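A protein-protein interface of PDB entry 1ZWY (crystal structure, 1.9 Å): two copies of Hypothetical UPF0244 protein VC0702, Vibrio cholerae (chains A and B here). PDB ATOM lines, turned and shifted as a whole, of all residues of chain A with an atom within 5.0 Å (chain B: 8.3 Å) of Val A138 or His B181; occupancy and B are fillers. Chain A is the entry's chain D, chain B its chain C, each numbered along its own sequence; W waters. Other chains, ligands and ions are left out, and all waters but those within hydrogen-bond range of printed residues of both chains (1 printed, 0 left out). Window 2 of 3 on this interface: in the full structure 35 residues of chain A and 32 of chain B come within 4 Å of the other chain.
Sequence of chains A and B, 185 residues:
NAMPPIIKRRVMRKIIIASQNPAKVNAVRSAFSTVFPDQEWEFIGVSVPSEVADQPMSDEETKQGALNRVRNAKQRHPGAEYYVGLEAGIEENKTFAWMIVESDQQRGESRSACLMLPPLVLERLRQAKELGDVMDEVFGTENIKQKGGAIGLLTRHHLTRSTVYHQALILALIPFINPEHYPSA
O of Leu A154 lies within hydrogen-bond range of ND2 of Asn B178 (2.8 Å).
O of Tyr B182 sits close to OE1 of Gln B106 (2.8 Å).
The side-chain amide nitrogen (ND2) of Asn B178 lies within hydrogen-bond range of the backbone carbonyl oxygen (O) of Ile B174 (2.8 Å).
Among the printed residues, merely in contact across the chains: Pro A118 with His B181 (3.3 Å), Pro A118 with Tyr B182 (3.4 Å), Pro A119 with His B181 (3.9 Å), Val A138 with His B181 (3.7 Å), Phe A139 with His B181 (3.5 Å), Leu A154 with Ile B174 (3.9 Å), Leu A154 with Ile B177 (3.2 Å) and Leu A154 with Tyr B182 (3.7 Å).
His B181 touches just these residues of chain A: Pro A118 (3.3 Å), Pro A119 (3.9 Å), Val A138 (3.7 Å) and Phe A139 (3.5 Å).
Of the printed residues of chain A, Asn B178 touches Leu A154 (2.8 Å).
Of the printed residues of chain B, Phe A139 touches His B181 (3.5 Å).
Printed residues of chain B within 4 Å of Leu A154: Ile B174 (3.9 Å), Ile B177 (3.2 Å), Asn B178 (2.8 Å) and Tyr B182 (3.7 Å).
Of the printed residues of chain B, Pro A119 touches His B181.
Asp A136 touches none of the printed residues of chain B.
The nearest printed residue of chain B that does not touch Pro A119 is Pro B183 (4.2 Å).
Of the 11 printed residues of chain B, 5 touch a printed residue of chain A.
Among the printed residues, no Asp or Glu carboxylate lies within 4 Å of a Lys or Arg side-chain nitrogen of the other chain.
No position is printed for both chains.
Of the 9 pairs that touch across the chains among the printed residues, none has its exchanged pair printed and touching as well.
Water W1 lies within hydrogen-bond range of O of His B181 (2.8 Å) and N of Leu A120 (3.2 Å).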
ATOM      1  N   PRO A 118     -25.316  18.346 -19.156  1.00  0.00           N
ATOM      2  CA  PRO A 118     -24.606  17.252 -19.796  1.00  0.00           C
ATOM      3  C   PRO A 118     -25.390  16.761 -21.036  1.00  0.00           C
ATOM      4  O   PRO A 118     -26.617  16.814 -21.034  1.00  0.00           O
ATOM      5  CB  PRO A 118     -24.607  16.129 -18.724  1.00  0.00           C
ATOM      6  CG  PRO A 118     -25.079  16.703 -17.509  1.00  0.00           C
ATOM      7  CD  PRO A 118     -25.734  18.026 -17.775  1.00  0.00           C
ATOM      8  N   PRO A 119     -24.694  16.268 -22.068  1.00  0.00           N
ATOM      9  CA  PRO A 119     -25.426  15.802 -23.242  1.00  0.00           C
ATOM     10  C   PRO A 119     -26.442  14.666 -22.951  1.00  0.00           C
ATOM     11  O   PRO A 119     -27.500  14.612 -23.589  1.00  0.00           O
ATOM     12  CB  PRO A 119     -24.311  15.357 -24.203  1.00  0.00           C
ATOM     13  CG  PRO A 119     -23.080  16.053 -23.700  1.00  0.00           C
ATOM     14  CD  PRO A 119     -23.232  16.131 -22.243  1.00  0.00           C
ATOM     15  N   LEU A 120     -26.176  13.802 -21.968  1.00  0.00           N
ATOM     16  CA  LEU A 120     -27.160  12.758 -21.597  1.00  0.00           C
ATOM     17  C   LEU A 120     -28.458  13.367 -21.026  1.00  0.00           C
ATOM     18  O   LEU A 120     -29.563  12.848 -21.258  1.00  0.00           O
ATOM     19  CB  LEU A 120     -26.578  11.775 -20.570  1.00  0.00           C
ATOM     20  CG  LEU A 120     -27.514  10.613 -20.155  1.00  0.00           C
ATOM     21  CD1 LEU A 120     -28.018   9.755 -21.371  1.00  0.00           C
ATOM     22  CD2 LEU A 120     -26.863   9.732 -19.112  1.00  0.00           C
ATOM     23  N   VAL A 121     -28.320  14.437 -20.245  1.00  0.00           N
ATOM     24  CA  VAL A 121     -29.516  15.171 -19.736  1.00  0.00           C
ATOM     25  C   VAL A 121     -30.380  15.710 -20.884  1.00  0.00           C
ATOM     26  O   VAL A 121     -31.617  15.541 -20.875  1.00  0.00           O
ATOM     27  CB  VAL A 121     -29.148  16.306 -18.748  1.00  0.00           C
ATOM     28  CG1 VAL A 121     -30.382  17.196 -18.434  1.00  0.00           C
ATOM     29  CG2 VAL A 121     -28.506  15.717 -17.430  1.00  0.00           C
ATOM     30  N   VAL A 134     -34.565  13.592 -14.513  1.00  0.00           N
ATOM     31  CA  VAL A 134     -33.433  13.312 -15.393  1.00  0.00           C
ATOM     32  C   VAL A 134     -32.124  13.561 -14.606  1.00  0.00           C
ATOM     33  O   VAL A 134     -31.158  12.809 -14.759  1.00  0.00           O
ATOM     34  CB  VAL A 134     -33.493  14.149 -16.682  1.00  0.00           C
ATOM     35  CG1 VAL A 134     -32.204  13.968 -17.501  1.00  0.00           C
ATOM     36  CG2 VAL A 134     -34.751  13.764 -17.527  1.00  0.00           C
ATOM     37  N   MET A 135     -32.127  14.557 -13.723  1.00  0.00           N
ATOM     38  CA  MET A 135     -30.935  14.852 -12.914  1.00  0.00           C
ATOM     39  C   MET A 135     -30.635  13.704 -11.963  1.00  0.00           C
ATOM     40  O   MET A 135     -29.486  13.290 -11.846  1.00  0.00           O
ATOM     41  CB  MET A 135     -31.060  16.159 -12.147  1.00  0.00           C
ATOM     42  CG  MET A 135     -31.177  17.401 -13.018  1.00  0.00           C
ATOM     43  SD  MET A 135     -29.545  17.698 -14.104  1.00  0.00           S
ATOM     44  CE  MET A 135     -29.293  19.700 -13.593  1.00  0.00           C
ATOM     45  N   ASP A 136     -31.680  13.151 -11.349  1.00  0.00           N
ATOM     46  CA  ASP A 136     -31.549  11.978 -10.471  1.00  0.00           C
ATOM     47  C   ASP A 136     -31.028  10.759 -11.210  1.00  0.00           C
ATOM     48  O   ASP A 136     -30.155  10.047 -10.682  1.00  0.00           O
ATOM     49  CB  ASP A 136     -32.881  11.652  -9.800  1.00  0.00           C
ATOM     50  CG  ASP A 136     -33.221  12.639  -8.705  1.00  0.00           C
ATOM     51  OD1 ASP A 136     -32.321  13.366  -8.222  1.00  0.00           O
ATOM     52  OD2 ASP A 136     -34.397  12.709  -8.339  1.00  0.00           O
ATOM     53  N   GLU A 137     -31.570  10.523 -12.411  1.00  0.00           N
ATOM     54  CA  GLU A 137     -31.082   9.441 -13.295  1.00  0.00           C
ATOM     55  C   GLU A 137     -29.597   9.575 -13.624  1.00  0.00           C
ATOM     56  O   GLU A 137     -28.842   8.602 -13.549  1.00  0.00           O
ATOM     57  CB  GLU A 137     -31.823   9.468 -14.631  1.00  0.00           C
ATOM     58  CG  GLU A 137     -33.273   9.031 -14.596  1.00  0.00           C
ATOM     59  CD  GLU A 137     -33.981   9.188 -15.970  1.00  0.00           C
ATOM     60  OE1 GLU A 137     -33.319   9.532 -16.994  1.00  0.00           O
ATOM     61  OE2 GLU A 137     -35.215   8.959 -16.013  1.00  0.00           O
ATOM     62  N   VAL A 138     -29.192  10.769 -14.032  1.00  0.00           N
ATOM     63  CA  VAL A 138     -27.850  10.981 -14.530  1.00  0.00           C
ATOM     64  C   VAL A 138     -26.801  11.056 -13.372  1.00  0.00           C
ATOM     65  O   VAL A 138     -25.757  10.443 -13.478  1.00  0.00           O
ATOM     66  CB  VAL A 138     -27.787  12.209 -15.461  1.00  0.00           C
ATOM     67  CG1 VAL A 138     -26.360  12.569 -15.772  1.00  0.00           C
ATOM     68  CG2 VAL A 138     -28.574  11.915 -16.793  1.00  0.00           C
ATOM     69  N   PHE A 139     -27.125  11.780 -12.286  1.00  0.00           N
ATOM     70  CA  PHE A 139     -26.238  11.951 -11.105  1.00  0.00           C
ATOM     71  C   PHE A 139     -26.523  11.052  -9.909  1.00  0.00           C
ATOM     72  O   PHE A 139     -25.646  10.824  -9.065  1.00  0.00           O
ATOM     73  CB  PHE A 139     -26.239  13.428 -10.679  1.00  0.00           C
ATOM     74  CG  PHE A 139     -25.820  14.336 -11.777  1.00  0.00           C
ATOM     75  CD1 PHE A 139     -24.486  14.394 -12.165  1.00  0.00           C
ATOM     76  CD2 PHE A 139     -26.757  15.071 -12.489  1.00  0.00           C
ATOM     77  CE1 PHE A 139     -24.089  15.201 -13.227  1.00  0.00           C
ATOM     78  CE2 PHE A 139     -26.370  15.887 -13.547  1.00  0.00           C
ATOM     79  CZ  PHE A 139     -25.035  15.932 -13.944  1.00  0.00           C
ATOM     80  N   GLY A 140     -27.749  10.559  -9.813  1.00  0.00           N
ATOM     81  CA  GLY A 140     -28.180   9.769  -8.677  1.00  0.00           C
ATOM     82  C   GLY A 140     -28.868  10.617  -7.645  1.00  0.00           C
ATOM     83  O   GLY A 140     -28.390  11.718  -7.293  1.00  0.00           O
ATOM     84  N   LEU A 154     -21.843  19.526  -9.060  1.00  0.00           N
ATOM     85  CA  LEU A 154     -21.000  19.837 -10.232  1.00  0.00           C
ATOM     86  C   LEU A 154     -19.867  20.858  -9.990  1.00  0.00           C
ATOM     87  O   LEU A 154     -18.843  20.845 -10.703  1.00  0.00           O
ATOM     88  CB  LEU A 154     -21.881  20.316 -11.377  1.00  0.00           C
ATOM     89  CG  LEU A 154     -22.831  19.269 -12.015  1.00  0.00           C
ATOM     90  CD1 LEU A 154     -23.797  19.934 -13.016  1.00  0.00           C
ATOM     91  CD2 LEU A 154     -22.050  18.120 -12.645  1.00  0.00           C
ATOM     92  N   GLN B 106     -12.485  20.198 -24.885  1.00  0.00           N
ATOM     93  CA  GLN B 106     -13.813  20.431 -24.334  1.00  0.00           C
ATOM     94  C   GLN B 106     -14.087  21.923 -24.110  1.00  0.00           C
ATOM     95  O   GLN B 106     -13.178  22.715 -24.042  1.00  0.00           O
ATOM     96  CB  GLN B 106     -13.963  19.624 -23.039  1.00  0.00           C
ATOM     97  CG  GLN B 106     -15.263  19.796 -22.303  1.00  0.00           C
ATOM     98  CD  GLN B 106     -16.480  19.239 -23.063  1.00  0.00           C
ATOM     99  OE1 GLN B 106     -17.087  18.276 -22.619  1.00  0.00           O
ATOM    100  NE2 GLN B 106     -16.847  19.864 -24.179  1.00  0.00           N
ATOM    101  N   ILE B 174     -17.472  23.775 -15.157  1.00  0.00           N
ATOM    102  CA  ILE B 174     -18.108  22.515 -14.775  1.00  0.00           C
ATOM    103  C   ILE B 174     -17.676  21.263 -15.582  1.00  0.00           C
ATOM    104  O   ILE B 174     -17.495  20.209 -14.982  1.00  0.00           O
ATOM    105  CB  ILE B 174     -19.636  22.661 -14.730  1.00  0.00           C
ATOM    106  CG1 ILE B 174     -20.054  23.325 -13.404  1.00  0.00           C
ATOM    107  CG2 ILE B 174     -20.344  21.317 -14.867  1.00  0.00           C
ATOM    108  CD1 ILE B 174     -21.566  23.743 -13.356  1.00  0.00           C
ATOM    109  N   PRO B 175     -17.567  21.354 -16.929  1.00  0.00           N
ATOM    110  CA  PRO B 175     -17.125  20.155 -17.686  1.00  0.00           C
ATOM    111  C   PRO B 175     -15.738  19.646 -17.342  1.00  0.00           C
ATOM    112  O   PRO B 175     -15.490  18.460 -17.420  1.00  0.00           O
ATOM    113  CB  PRO B 175     -17.163  20.630 -19.156  1.00  0.00           C
ATOM    114  CG  PRO B 175     -18.208  21.735 -19.146  1.00  0.00           C
ATOM    115  CD  PRO B 175     -17.961  22.448 -17.846  1.00  0.00           C
ATOM    116  N   ILE B 177     -14.369  20.034 -14.368  1.00  0.00           N
ATOM    117  CA  ILE B 177     -14.532  19.468 -13.032  1.00  0.00           C
ATOM    118  C   ILE B 177     -15.140  18.051 -13.163  1.00  0.00           C
ATOM    119  O   ILE B 177     -14.831  17.168 -12.369  1.00  0.00           O
ATOM    120  CB  ILE B 177     -15.446  20.391 -12.155  1.00  0.00           C
ATOM    121  CG1 ILE B 177     -14.772  21.722 -11.842  1.00  0.00           C
ATOM    122  CG2 ILE B 177     -15.827  19.741 -10.815  1.00  0.00           C
ATOM    123  CD1 ILE B 177     -15.687  22.713 -11.166  1.00  0.00           C
ATOM    124  N   ASN B 178     -16.014  17.845 -14.155  1.00  0.00           N
ATOM    125  CA  ASN B 178     -16.822  16.614 -14.253  1.00  0.00           C
ATOM    126  C   ASN B 178     -16.684  15.858 -15.592  1.00  0.00           C
ATOM    127  O   ASN B 178     -17.674  15.660 -16.307  1.00  0.00           O
ATOM    128  CB  ASN B 178     -18.288  16.940 -13.978  1.00  0.00           C
ATOM    129  CG  ASN B 178     -18.476  17.652 -12.672  1.00  0.00           C
ATOM    130  OD1 ASN B 178     -18.554  17.018 -11.615  1.00  0.00           O
ATOM    131  ND2 ASN B 178     -18.505  18.988 -12.718  1.00  0.00           N
ATOM    132  N   PRO B 179     -15.453  15.441 -15.938  1.00  0.00           N
ATOM    133  CA  PRO B 179     -15.242  14.884 -17.269  1.00  0.00           C
ATOM    134  C   PRO B 179     -16.115  13.667 -17.581  1.00  0.00           C
ATOM    135  O   PRO B 179     -16.523  13.493 -18.736  1.00  0.00           O
ATOM    136  CB  PRO B 179     -13.741  14.485 -17.252  1.00  0.00           C
ATOM    137  CG  PRO B 179     -13.400  14.364 -15.804  1.00  0.00           C
ATOM    138  CD  PRO B 179     -14.189  15.473 -15.170  1.00  0.00           C
ATOM    139  N   GLU B 180     -16.414  12.846 -16.567  1.00  0.00           N
ATOM    140  CA  GLU B 180     -17.248  11.660 -16.764  1.00  0.00           C
ATOM    141  C   GLU B 180     -18.652  12.046 -17.249  1.00  0.00           C
ATOM    142  O   GLU B 180     -19.280  11.317 -18.035  1.00  0.00           O
ATOM    143  CB  GLU B 180     -17.383  10.821 -15.480  1.00  0.00           C
ATOM    144  CG  GLU B 180     -16.401  11.135 -14.324  1.00  0.00           C
ATOM    145  CD  GLU B 180     -16.809  12.375 -13.503  1.00  0.00           C
ATOM    146  OE1 GLU B 180     -17.719  12.275 -12.657  1.00  0.00           O
ATOM    147  OE2 GLU B 180     -16.207  13.436 -13.689  1.00  0.00           O
ATOM    148  N   HIS B 181     -19.142  13.194 -16.800  1.00  0.00           N
ATOM    149  CA  HIS B 181     -20.481  13.644 -17.208  1.00  0.00           C
ATOM    150  C   HIS B 181     -20.512  14.534 -18.443  1.00  0.00           C
ATOM    151  O   HIS B 181     -21.576  14.766 -19.028  1.00  0.00           O
ATOM    152  CB  HIS B 181     -21.162  14.362 -16.035  1.00  0.00           C
ATOM    153  CG  HIS B 181     -21.538  13.424 -14.940  1.00  0.00           C
ATOM    154  ND1 HIS B 181     -20.947  13.450 -13.699  1.00  0.00           N
ATOM    155  CD2 HIS B 181     -22.455  12.431 -14.905  1.00  0.00           C
ATOM    156  CE1 HIS B 181     -21.478  12.503 -12.943  1.00  0.00           C
ATOM    157  NE2 HIS B 181     -22.387  11.864 -13.657  1.00  0.00           N
ATOM    158  N   TYR B 182     -19.341  15.048 -18.813  1.00  0.00           N
ATOM    159  CA  TYR B 182     -19.237  15.954 -19.945  1.00  0.00           C
ATOM    160  C   TYR B 182     -18.155  15.434 -20.883  1.00  0.00           C
ATOM    161  O   TYR B 182     -17.067  15.998 -20.926  1.00  0.00           O
ATOM    162  CB  TYR B 182     -18.912  17.405 -19.490  1.00  0.00           C
ATOM    163  CG  TYR B 182     -20.057  18.070 -18.739  1.00  0.00           C
ATOM    164  CD1 TYR B 182     -20.257  17.822 -17.384  1.00  0.00           C
ATOM    165  CD2 TYR B 182     -20.923  18.941 -19.390  1.00  0.00           C
ATOM    166  CE1 TYR B 182     -21.288  18.425 -16.686  1.00  0.00           C
ATOM    167  CE2 TYR B 182     -21.980  19.551 -18.707  1.00  0.00           C
ATOM    168  CZ  TYR B 182     -22.143  19.282 -17.337  1.00  0.00           C
ATOM    169  OH  TYR B 182     -23.159  19.850 -16.638  1.00  0.00           O
ATOM    170  N   PRO B 183     -18.462  14.362 -21.645  1.00  0.00           N
ATOM    171  CA  PRO B 183     -17.426  13.744 -22.495  1.00  0.00           C
ATOM    172  C   PRO B 183     -17.122  14.679 -23.660  1.00  0.00           C
ATOM    173  O   PRO B 183     -17.997  15.414 -24.095  1.00  0.00           O
ATOM    174  CB  PRO B 183     -18.092  12.432 -22.975  1.00  0.00           C
ATOM    175  CG  PRO B 183     -19.551  12.717 -22.948  1.00  0.00           C
ATOM    176  CD  PRO B 183     -19.786  13.733 -21.816  1.00  0.00           C
ATOM    177  N   SER B 184     -15.895  14.683 -24.146  1.00  0.00           N
ATOM    178  CA  SER B 184     -15.562  15.590 -25.234  1.00  0.00           C
ATOM    179  C   SER B 184     -16.089  15.128 -26.609  1.00  0.00           C
ATOM    180  O   SER B 184     -16.117  15.920 -27.563  1.00  0.00           O
ATOM    181  CB  SER B 184     -14.067  15.806 -25.247  1.00  0.00           C
ATOM    182  OG  SER B 184     -13.416  14.566 -25.084  1.00  0.00           O
HETATM  183  O   HOH W   1     -23.646  13.196 -20.123  1.00  0.00           O
